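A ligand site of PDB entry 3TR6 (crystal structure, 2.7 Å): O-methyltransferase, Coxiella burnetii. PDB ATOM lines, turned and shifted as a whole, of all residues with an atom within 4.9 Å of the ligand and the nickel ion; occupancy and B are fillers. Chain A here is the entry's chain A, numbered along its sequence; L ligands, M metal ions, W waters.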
ATOM      1  N   MET A  46       5.546 -28.209 -36.736  1.00  0.00           N
ATOM      2  CA  MET A  46       4.708 -28.935 -35.785  1.00  0.00           C
ATOM      3  C   MET A  46       3.608 -28.045 -35.202  1.00  0.00           C
ATOM      4  O   MET A  46       2.866 -28.460 -34.309  1.00  0.00           O
ATOM      5  CB  MET A  46       5.550 -29.598 -34.683  1.00  0.00           C
ATOM      6  CG  MET A  46       6.486 -28.669 -33.924  1.00  0.00           C
ATOM      7  SD  MET A  46       7.638 -29.629 -32.649  1.00  0.00           S
ATOM      8  CE  MET A  46       7.224 -31.454 -33.185  1.00  0.00           C
ATOM      9  N   GLN A  47       3.486 -26.832 -35.722  1.00  0.00           N
ATOM     10  CA  GLN A  47       2.437 -25.922 -35.302  1.00  0.00           C
ATOM     11  C   GLN A  47       1.074 -26.380 -35.798  1.00  0.00           C
ATOM     12  O   GLN A  47       0.947 -26.954 -36.885  1.00  0.00           O
ATOM     13  CB  GLN A  47       2.726 -24.503 -35.787  1.00  0.00           C
ATOM     14  CG  GLN A  47       1.837 -23.434 -35.173  1.00  0.00           C
ATOM     15  CD  GLN A  47       2.201 -22.039 -35.651  1.00  0.00           C
ATOM     16  OE1 GLN A  47       2.674 -21.856 -36.769  1.00  0.00           O
ATOM     17  NE2 GLN A  47       1.988 -21.051 -34.793  1.00  0.00           N
ATOM     18  N   THR A  48       0.038 -26.135 -34.993  1.00  0.00           N
ATOM     19  CA  THR A  48      -1.311 -26.553 -35.345  1.00  0.00           C
ATOM     20  C   THR A  48      -1.799 -25.809 -36.582  1.00  0.00           C
ATOM     21  O   THR A  48      -1.624 -24.587 -36.691  1.00  0.00           O
ATOM     22  CB  THR A  48      -2.285 -26.322 -34.172  1.00  0.00           C
ATOM     23  OG1 THR A  48      -1.871 -27.099 -33.043  1.00  0.00           O
ATOM     24  CG2 THR A  48      -3.697 -26.728 -34.554  1.00  0.00           C
ATOM     25  N   ASP A  70      -4.452 -28.294 -22.759  1.00  0.00           N
ATOM     26  CA  ASP A  70      -3.753 -28.218 -24.022  1.00  0.00           C
ATOM     27  C   ASP A  70      -2.387 -28.881 -23.873  1.00  0.00           C
ATOM     28  O   ASP A  70      -1.454 -28.293 -23.339  1.00  0.00           O
ATOM     29  CB  ASP A  70      -3.608 -26.752 -24.455  1.00  0.00           C
ATOM     30  CG  ASP A  70      -2.791 -26.583 -25.712  1.00  0.00           C
ATOM     31  OD1 ASP A  70      -3.289 -26.938 -26.798  1.00  0.00           O
ATOM     32  OD2 ASP A  70      -1.649 -26.081 -25.627  1.00  0.00           O
ATOM     33  N   GLY A  72       0.959 -29.894 -25.192  1.00  0.00           N
ATOM     34  CA  GLY A  72       1.884 -29.524 -26.252  1.00  0.00           C
ATOM     35  C   GLY A  72       1.726 -28.077 -26.658  1.00  0.00           C
ATOM     36  O   GLY A  72       1.058 -27.771 -27.647  1.00  0.00           O
ATOM     37  N   THR A  73       2.354 -27.174 -25.906  1.00  0.00           N
ATOM     38  CA  THR A  73       2.168 -25.748 -26.091  1.00  0.00           C
ATOM     39  C   THR A  73       2.859 -25.205 -27.340  1.00  0.00           C
ATOM     40  O   THR A  73       2.270 -24.434 -28.093  1.00  0.00           O
ATOM     41  CB  THR A  73       2.718 -24.955 -24.890  1.00  0.00           C
ATOM     42  OG1 THR A  73       2.337 -25.589 -23.664  1.00  0.00           O
ATOM     43  CG2 THR A  73       2.185 -23.523 -24.916  1.00  0.00           C
ATOM     44  N   PHE A  74       4.103 -25.622 -27.543  1.00  0.00           N
ATOM     45  CA  PHE A  74       4.951 -25.012 -28.556  1.00  0.00           C
ATOM     46  C   PHE A  74       4.917 -23.500 -28.359  1.00  0.00           C
ATOM     47  O   PHE A  74       5.198 -23.001 -27.276  1.00  0.00           O
ATOM     48  CB  PHE A  74       4.488 -25.382 -29.963  1.00  0.00           C
ATOM     49  CG  PHE A  74       5.509 -25.085 -31.030  1.00  0.00           C
ATOM     50  CD1 PHE A  74       6.845 -24.934 -30.711  1.00  0.00           C
ATOM     51  CD2 PHE A  74       5.117 -24.940 -32.357  1.00  0.00           C
ATOM     52  CE1 PHE A  74       7.789 -24.660 -31.689  1.00  0.00           C
ATOM     53  CE2 PHE A  74       6.044 -24.662 -33.346  1.00  0.00           C
ATOM     54  CZ  PHE A  74       7.391 -24.518 -33.008  1.00  0.00           C
ATOM     55  N   THR A  75       4.561 -22.757 -29.404  1.00  0.00           N
ATOM     56  CA  THR A  75       4.439 -21.300 -29.282  1.00  0.00           C
ATOM     57  C   THR A  75       3.003 -20.879 -28.974  1.00  0.00           C
ATOM     58  O   THR A  75       2.650 -19.707 -29.081  1.00  0.00           O
ATOM     59  CB  THR A  75       4.961 -20.572 -30.535  1.00  0.00           C
ATOM     60  OG1 THR A  75       4.241 -21.015 -31.692  1.00  0.00           O
ATOM     61  CG2 THR A  75       6.450 -20.852 -30.737  1.00  0.00           C
ATOM     62  N   GLY A  76       2.184 -21.862 -28.605  1.00  0.00           N
ATOM     63  CA  GLY A  76       0.862 -21.603 -28.049  1.00  0.00           C
ATOM     64  C   GLY A  76      -0.267 -21.284 -29.002  1.00  0.00           C
ATOM     65  O   GLY A  76      -1.216 -20.597 -28.618  1.00  0.00           O
ATOM     66  N   TYR A  77      -0.192 -21.782 -30.235  1.00  0.00           N
ATOM     67  CA  TYR A  77      -1.238 -21.506 -31.219  1.00  0.00           C
ATOM     68  C   TYR A  77      -2.589 -22.099 -30.815  1.00  0.00           C
ATOM     69  O   TYR A  77      -3.609 -21.408 -30.771  1.00  0.00           O
ATOM     70  CB  TYR A  77      -0.841 -21.984 -32.621  1.00  0.00           C
ATOM     71  CG  TYR A  77      -1.740 -21.449 -33.724  1.00  0.00           C
ATOM     72  CD1 TYR A  77      -1.377 -20.328 -34.463  1.00  0.00           C
ATOM     73  CD2 TYR A  77      -2.947 -22.062 -34.017  1.00  0.00           C
ATOM     74  CE1 TYR A  77      -2.199 -19.835 -35.458  1.00  0.00           C
ATOM     75  CE2 TYR A  77      -3.769 -21.579 -35.016  1.00  0.00           C
ATOM     76  CZ  TYR A  77      -3.395 -20.465 -35.736  1.00  0.00           C
ATOM     77  OH  TYR A  77      -4.229 -19.988 -36.720  1.00  0.00           O
ATOM     78  N   SER A  78      -2.606 -23.398 -30.511  1.00  0.00           N
ATOM     79  CA  SER A  78      -3.844 -24.074 -30.145  1.00  0.00           C
ATOM     80  C   SER A  78      -4.362 -23.610 -28.788  1.00  0.00           C
ATOM     81  O   SER A  78      -5.564 -23.524 -28.561  1.00  0.00           O
ATOM     82  CB  SER A  78      -3.647 -25.591 -30.142  1.00  0.00           C
ATOM     83  OG  SER A  78      -2.601 -25.980 -29.279  1.00  0.00           O
ATOM     84  N   CYS A  95       0.455 -27.495 -21.555  1.00  0.00           N
ATOM     85  CA  CYS A  95       1.605 -28.264 -21.099  1.00  0.00           C
ATOM     86  C   CYS A  95       2.713 -28.301 -22.136  1.00  0.00           C
ATOM     87  O   CYS A  95       2.470 -28.511 -23.329  1.00  0.00           O
ATOM     88  CB  CYS A  95       1.186 -29.683 -20.751  1.00  0.00           C
ATOM     89  SG  CYS A  95      -0.245 -29.797 -19.675  1.00  0.00           S
ATOM     90  N   ASP A  96       3.950 -28.120 -21.671  1.00  0.00           N
ATOM     91  CA  ASP A  96       5.121 -28.282 -22.500  1.00  0.00           C
ATOM     92  C   ASP A  96       6.338 -28.380 -21.593  1.00  0.00           C
ATOM     93  O   ASP A  96       6.243 -28.137 -20.394  1.00  0.00           O
ATOM     94  CB  ASP A  96       5.268 -27.125 -23.492  1.00  0.00           C
ATOM     95  CG  ASP A  96       6.022 -27.523 -24.751  1.00  0.00           C
ATOM     96  OD1 ASP A  96       7.081 -28.171 -24.632  1.00  0.00           O
ATOM     97  OD2 ASP A  96       5.557 -27.196 -25.855  1.00  0.00           O
ATOM     98  N   VAL A  97       7.481 -28.716 -22.168  1.00  0.00           N
ATOM     99  CA  VAL A  97       8.706 -28.836 -21.395  1.00  0.00           C
ATOM    100  C   VAL A  97       9.762 -27.871 -21.946  1.00  0.00           C
ATOM    101  O   VAL A  97      10.846 -27.748 -21.382  1.00  0.00           O
ATOM    102  CB  VAL A  97       9.249 -30.273 -21.441  1.00  0.00           C
ATOM    103  CG1 VAL A  97       9.835 -30.571 -22.815  1.00  0.00           C
ATOM    104  CG2 VAL A  97      10.274 -30.495 -20.347  1.00  0.00           C
ATOM    105  N   ASP A  98       9.417 -27.197 -23.036  1.00  0.00           N
ATOM    106  CA  ASP A  98      10.363 -26.310 -23.712  1.00  0.00           C
ATOM    107  C   ASP A  98      10.173 -24.858 -23.302  1.00  0.00           C
ATOM    108  O   ASP A  98       9.104 -24.274 -23.506  1.00  0.00           O
ATOM    109  CB  ASP A  98      10.206 -26.456 -25.235  1.00  0.00           C
ATOM    110  CG  ASP A  98      11.273 -25.717 -26.007  1.00  0.00           C
ATOM    111  OD1 ASP A  98      12.400 -26.249 -26.132  1.00  0.00           O
ATOM    112  OD2 ASP A  98      11.002 -24.606 -26.509  1.00  0.00           O
ATOM    113  N   SER A 101      10.063 -21.855 -26.522  1.00  0.00           N
ATOM    114  CA  SER A 101       8.796 -21.703 -27.236  1.00  0.00           C
ATOM    115  C   SER A 101       7.652 -21.199 -26.349  1.00  0.00           C
ATOM    116  O   SER A 101       6.855 -20.369 -26.778  1.00  0.00           O
ATOM    117  CB  SER A 101       8.400 -23.007 -27.927  1.00  0.00           C
ATOM    118  OG  SER A 101       8.286 -24.064 -27.002  1.00  0.00           O
ATOM    119  N   SER A 123       6.511 -28.721 -17.521  1.00  0.00           N
ATOM    120  CA  SER A 123       7.112 -29.965 -17.071  1.00  0.00           C
ATOM    121  C   SER A 123       6.537 -31.079 -17.916  1.00  0.00           C
ATOM    122  O   SER A 123       5.554 -30.866 -18.628  1.00  0.00           O
ATOM    123  CB  SER A 123       6.810 -30.208 -15.584  1.00  0.00           C
ATOM    124  OG  SER A 123       5.684 -31.045 -15.417  1.00  0.00           O
ATOM    125  N   PRO A 124       7.135 -32.278 -17.856  1.00  0.00           N
ATOM    126  CA  PRO A 124       6.564 -33.397 -18.634  1.00  0.00           C
ATOM    127  C   PRO A 124       5.057 -33.487 -18.444  1.00  0.00           C
ATOM    128  O   PRO A 124       4.588 -33.439 -17.313  1.00  0.00           O
ATOM    129  CB  PRO A 124       7.261 -34.618 -18.024  1.00  0.00           C
ATOM    130  CG  PRO A 124       8.579 -34.102 -17.567  1.00  0.00           C
ATOM    131  CD  PRO A 124       8.335 -32.680 -17.104  1.00  0.00           C
ATOM    132  N   ALA A 125       4.315 -33.598 -19.544  1.00  0.00           N
ATOM    133  CA  ALA A 125       2.858 -33.682 -19.483  1.00  0.00           C
ATOM    134  C   ALA A 125       2.430 -34.875 -18.637  1.00  0.00           C
ATOM    135  O   ALA A 125       1.450 -34.828 -17.904  1.00  0.00           O
ATOM    136  CB  ALA A 125       2.274 -33.787 -20.879  1.00  0.00           C
ATOM    137  N   TYR A 145      -6.899 -31.547 -25.556  1.00  0.00           N
ATOM    138  CA  TYR A 145      -6.257 -31.604 -26.861  1.00  0.00           C
ATOM    139  C   TYR A 145      -4.842 -32.165 -26.727  1.00  0.00           C
ATOM    140  O   TYR A 145      -3.977 -31.544 -26.114  1.00  0.00           O
ATOM    141  CB  TYR A 145      -6.227 -30.203 -27.483  1.00  0.00           C
ATOM    142  CG  TYR A 145      -5.521 -30.117 -28.829  1.00  0.00           C
ATOM    143  CD1 TYR A 145      -5.872 -30.948 -29.882  1.00  0.00           C
ATOM    144  CD2 TYR A 145      -4.530 -29.165 -29.041  1.00  0.00           C
ATOM    145  CE1 TYR A 145      -5.227 -30.851 -31.112  1.00  0.00           C
ATOM    146  CE2 TYR A 145      -3.890 -29.062 -30.260  1.00  0.00           C
ATOM    147  CZ  TYR A 145      -4.239 -29.898 -31.301  1.00  0.00           C
ATOM    148  OH  TYR A 145      -3.591 -29.788 -32.511  1.00  0.00           O
ATOM    149  N   ASP A 147      -1.395 -33.071 -28.270  1.00  0.00           N
ATOM    150  CA  ASP A 147      -0.546 -32.695 -29.398  1.00  0.00           C
ATOM    151  C   ASP A 147       0.906 -32.462 -28.960  1.00  0.00           C
ATOM    152  O   ASP A 147       1.486 -31.407 -29.234  1.00  0.00           O
ATOM    153  CB  ASP A 147      -1.130 -31.470 -30.105  1.00  0.00           C
ATOM    154  CG  ASP A 147      -0.382 -31.114 -31.369  1.00  0.00           C
ATOM    155  OD1 ASP A 147      -0.575 -29.984 -31.869  1.00  0.00           O
ATOM    156  OD2 ASP A 147       0.395 -31.955 -31.850  1.00  0.00           O
ATOM    157  N   ALA A 148       1.487 -33.441 -28.280  1.00  0.00           N
ATOM    158  CA  ALA A 148       2.869 -33.352 -27.832  1.00  0.00           C
ATOM    159  C   ALA A 148       3.715 -34.483 -28.424  1.00  0.00           C
ATOM    160  O   ALA A 148       3.555 -34.830 -29.593  1.00  0.00           O
ATOM    161  CB  ALA A 148       2.929 -33.387 -26.308  1.00  0.00           C
ATOM    162  N   ASP A 149       4.609 -35.050 -27.625  1.00  0.00           N
ATOM    163  CA  ASP A 149       5.427 -36.170 -28.077  1.00  0.00           C
ATOM    164  C   ASP A 149       4.538 -37.369 -28.419  1.00  0.00           C
ATOM    165  O   ASP A 149       3.760 -37.835 -27.586  1.00  0.00           O
ATOM    166  CB  ASP A 149       6.486 -36.551 -27.043  1.00  0.00           C
ATOM    167  CG  ASP A 149       5.920 -36.634 -25.630  1.00  0.00           C
ATOM    168  OD1 ASP A 149       5.266 -35.661 -25.189  1.00  0.00           O
ATOM    169  OD2 ASP A 149       6.137 -37.670 -24.958  1.00  0.00           O
ATOM    170  N   LYS A 150       4.648 -37.858 -29.648  1.00  0.00           N
ATOM    171  CA  LYS A 150       3.729 -38.884 -30.156  1.00  0.00           C
ATOM    172  C   LYS A 150       3.907 -40.244 -29.480  1.00  0.00           C
ATOM    173  O   LYS A 150       2.981 -41.045 -29.436  1.00  0.00           O
ATOM    174  CB  LYS A 150       3.852 -39.024 -31.674  1.00  0.00           C
ATOM    175  CG  LYS A 150       3.779 -37.700 -32.429  1.00  0.00           C
ATOM    176  CD  LYS A 150       2.576 -36.863 -32.009  1.00  0.00           C
ATOM    177  CE  LYS A 150       2.607 -35.496 -32.683  1.00  0.00           C
ATOM    178  NZ  LYS A 150       1.683 -34.510 -32.048  1.00  0.00           N
ATOM    179  N   TYR A 156      -1.190 -40.382 -22.614  1.00  0.00           N
ATOM    180  CA  TYR A 156      -1.965 -39.145 -22.518  1.00  0.00           C
ATOM    181  C   TYR A 156      -3.454 -39.373 -22.746  1.00  0.00           C
ATOM    182  O   TYR A 156      -4.294 -38.735 -22.102  1.00  0.00           O
ATOM    183  CB  TYR A 156      -1.448 -38.114 -23.528  1.00  0.00           C
ATOM    184  CG  TYR A 156      -0.010 -37.710 -23.337  1.00  0.00           C
ATOM    185  CD1 TYR A 156       0.572 -37.723 -22.079  1.00  0.00           C
ATOM    186  CD2 TYR A 156       0.758 -37.306 -24.424  1.00  0.00           C
ATOM    187  CE1 TYR A 156       1.893 -37.343 -21.906  1.00  0.00           C
ATOM    188  CE2 TYR A 156       2.072 -36.923 -24.257  1.00  0.00           C
ATOM    189  CZ  TYR A 156       2.639 -36.947 -23.000  1.00  0.00           C
ATOM    190  OH  TYR A 156       3.950 -36.568 -22.849  1.00  0.00           O
ATOM    191  N   ASP A 173      -4.337 -34.908 -32.433  1.00  0.00           N
ATOM    192  CA  ASP A 173      -3.804 -34.480 -33.713  1.00  0.00           C
ATOM    193  C   ASP A 173      -2.815 -35.506 -34.275  1.00  0.00           C
ATOM    194  O   ASP A 173      -2.333 -36.382 -33.552  1.00  0.00           O
ATOM    195  CB  ASP A 173      -3.121 -33.116 -33.569  1.00  0.00           C
ATOM    196  CG  ASP A 173      -2.743 -32.502 -34.909  1.00  0.00           C
ATOM    197  OD1 ASP A 173      -3.205 -33.010 -35.962  1.00  0.00           O
ATOM    198  OD2 ASP A 173      -2.000 -31.501 -34.910  1.00  0.00           O
ATOM    199  N   ASN A 174      -2.525 -35.391 -35.571  1.00  0.00           N
ATOM    200  CA  ASN A 174      -1.486 -36.186 -36.229  1.00  0.00           C
ATOM    201  C   ASN A 174      -1.744 -37.689 -36.276  1.00  0.00           C
ATOM    202  O   ASN A 174      -0.810 -38.486 -36.268  1.00  0.00           O
ATOM    203  CB  ASN A 174      -0.112 -35.919 -35.602  1.00  0.00           C
ATOM    204  CG  ASN A 174       0.259 -34.449 -35.612  1.00  0.00           C
ATOM    205  OD1 ASN A 174       0.594 -33.874 -36.659  1.00  0.00           O
ATOM    206  ND2 ASN A 174       0.211 -33.821 -34.441  1.00  0.00           N
HETATM  207  N1  LIG L   1      -0.417 -27.534 -30.201  1.00  0.00           N
HETATM  208  C1  LIG L   1       0.866 -26.956 -30.506  1.00  0.00           C
HETATM  209  C2  LIG L   1       1.802 -27.974 -31.117  1.00  0.00           C
HETATM  210  C3  LIG L   1       2.972 -28.416 -30.259  1.00  0.00           C
HETATM  211  S1  LIG L   1       4.215 -29.451 -31.026  1.00  0.00           S
HETATM  212  C4  LIG L   1       0.693 -25.816 -31.446  1.00  0.00           C
HETATM  213  O1  LIG L   1       1.688 -25.407 -32.110  1.00  0.00           O
HETATM  214  O2  LIG L   1      -0.432 -25.262 -31.598  1.00  0.00           O
HETATM  215  C5  LIG L   1       4.918 -30.552 -29.815  1.00  0.00           C
HETATM  216  C6  LIG L   1       5.269 -29.986 -28.549  1.00  0.00           C
HETATM  217  O3  LIG L   1       5.300 -31.049 -27.529  1.00  0.00           O
HETATM  218  C7  LIG L   1       6.624 -29.405 -28.589  1.00  0.00           C
HETATM  219  O4  LIG L   1       6.561 -28.082 -28.237  1.00  0.00           O
HETATM  220  C8  LIG L   1       7.402 -30.155 -27.594  1.00  0.00           C
HETATM  221  O5  LIG L   1       8.247 -29.328 -26.903  1.00  0.00           O
HETATM  222  C9  LIG L   1       6.361 -30.700 -26.689  1.00  0.00           C
HETATM  223  N2  LIG L   1       6.744 -31.859 -25.872  1.00  0.00           N
HETATM  224  C10 LIG L   1       7.549 -32.863 -26.237  1.00  0.00           C
HETATM  225  N3  LIG L   1       7.636 -33.718 -25.201  1.00  0.00           N
HETATM  226  C11 LIG L   1       6.889 -33.247 -24.185  1.00  0.00           C
HETATM  227  C12 LIG L   1       6.610 -33.694 -22.890  1.00  0.00           C
HETATM  228  N4  LIG L   1       7.179 -34.920 -22.404  1.00  0.00           N
HETATM  229  N5  LIG L   1       5.789 -32.971 -22.107  1.00  0.00           N
HETATM  230  C13 LIG L   1       5.253 -31.828 -22.547  1.00  0.00           C
HETATM  231  N6  LIG L   1       5.506 -31.363 -23.776  1.00  0.00           N
HETATM  232  C14 LIG L   1       6.309 -32.055 -24.612  1.00  0.00           C
HETATM  233 NI    NI M   1       0.436 -31.306 -34.346  1.00  0.00          NI
HETATM  234  O   HOH W   1       5.664 -36.659 -20.622  1.00  0.00           O
HETATM  235  O   HOH W   2       1.867 -22.748 -31.944  1.00  0.00           O
HETATM  236  O   HOH W   3       3.086 -31.944 -33.193  1.00  0.00           O
HETATM  237  O   HOH W   4      11.143 -30.161 -26.412  1.00  0.00           O
HETATM  238  O   HOH W   5       8.700 -37.392 -23.207  1.00  0.00           O
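The nickel ion is bound by OD2 of Asp 173 (2.5 Å), ND2 of Asn 174 (2.5 Å) and OD2 of Asp 147 (2.6 Å).
The nickel ion has three donor atoms within binding distance.
Water W1 lies within hydrogen-bond range of OH of Tyr 156 (2.8 Å) and N4 of the ligand (2.9 Å).
Water W3 lies within hydrogen-bond range of NZ of Lys 150 (3.1 Å) and S1 of the ligand (3.5 Å).
Water W5 bridges a nitrogen (N4) of the ligand and the side-chain carboxylate of Asp 149.
Residues that only touch the nickel ion: Met 46.
The side-chain carboxylate (OD2) of Asp 173 lies close to the side-chain hydroxyl (OH) of Tyr 145, 3.3 Å away.
The side-chain amino group (NZ) of Lys 150 lies close to the side-chain carboxylate (OD2) of Asp 147, at 2.9 Å.
The backbone NH (N) of Thr 73 is in hydrogen-bond range of the side-chain carboxylate (OD2) of Asp 96 (3.2 Å).
The backbone NH (N) of Ser 123 sits at hydrogen-bond distance from the backbone carbonyl oxygen (O) of Asp 96 (2.9 Å).
OG1 of Thr 48 sits at hydrogen-bond distance from OH of Tyr 145 (3.2 Å).
The side-chain hydroxyl (OG) of Ser 78 is in hydrogen-bond range of the side-chain carboxylate (OD1) of Asp 70 (2.7 Å).
The backbone carbonyl oxygen of Cys 95 is in hydrogen-bond range of the backbone NH of Gly 72.
O of Phe 74 lies close to OG of Ser 101 (3.3 Å).
A sulfur (S1) of the ligand lies close to the backbone carbonyl oxygen (O) of Met 46, 3.7 Å away.
Gln 47 touches the ligand (CA to O1, 3.3 Å).
Thr 73 touches the ligand.
Phe 74 touches the ligand (CB to C3, 3.4 Å).
CB of Tyr 77 touches O2 of the ligand, at 3.5 Å.
Val 97 touches the ligand.
CB of Asp 98 touches O5 of the ligand, 3.9 Å away.
Pro 124 touches the ligand (CA to N5, 3.6 Å).
Tyr 145 touches the ligand.
Ala 148 touches the ligand.
Tyr 156 touches the ligand.
N1 of the ligand lies within salt-bridge range of OD1 of Asp 147 (3.0 Å).
OD2 of Asp 96 is in hydrogen-bond range of O4 of the ligand (2.7 Å).
The backbone NH (N) of Thr 48 lies within hydrogen-bond range of an oxygen (O1) of the ligand (3.4 Å).
O2 of the ligand lies within hydrogen-bond range of OG1 of Thr 48.
N of Ser 78 lies within hydrogen-bond range of O2 of the ligand (3.1 Å).
The side-chain hydroxyl (OG) of Ser 78 is in hydrogen-bond range of a nitrogen (N1) of the ligand, 2.8 Å away.
The backbone carbonyl oxygen (O) of Gly 72 lies within hydrogen-bond range of a nitrogen (N1) of the ligand (3.0 Å).
N5 of the ligand is in hydrogen-bond range of N of Ala 125 (3.0 Å).
N4 of the ligand lies close to OD1 of Asp 149 (3.5 Å).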
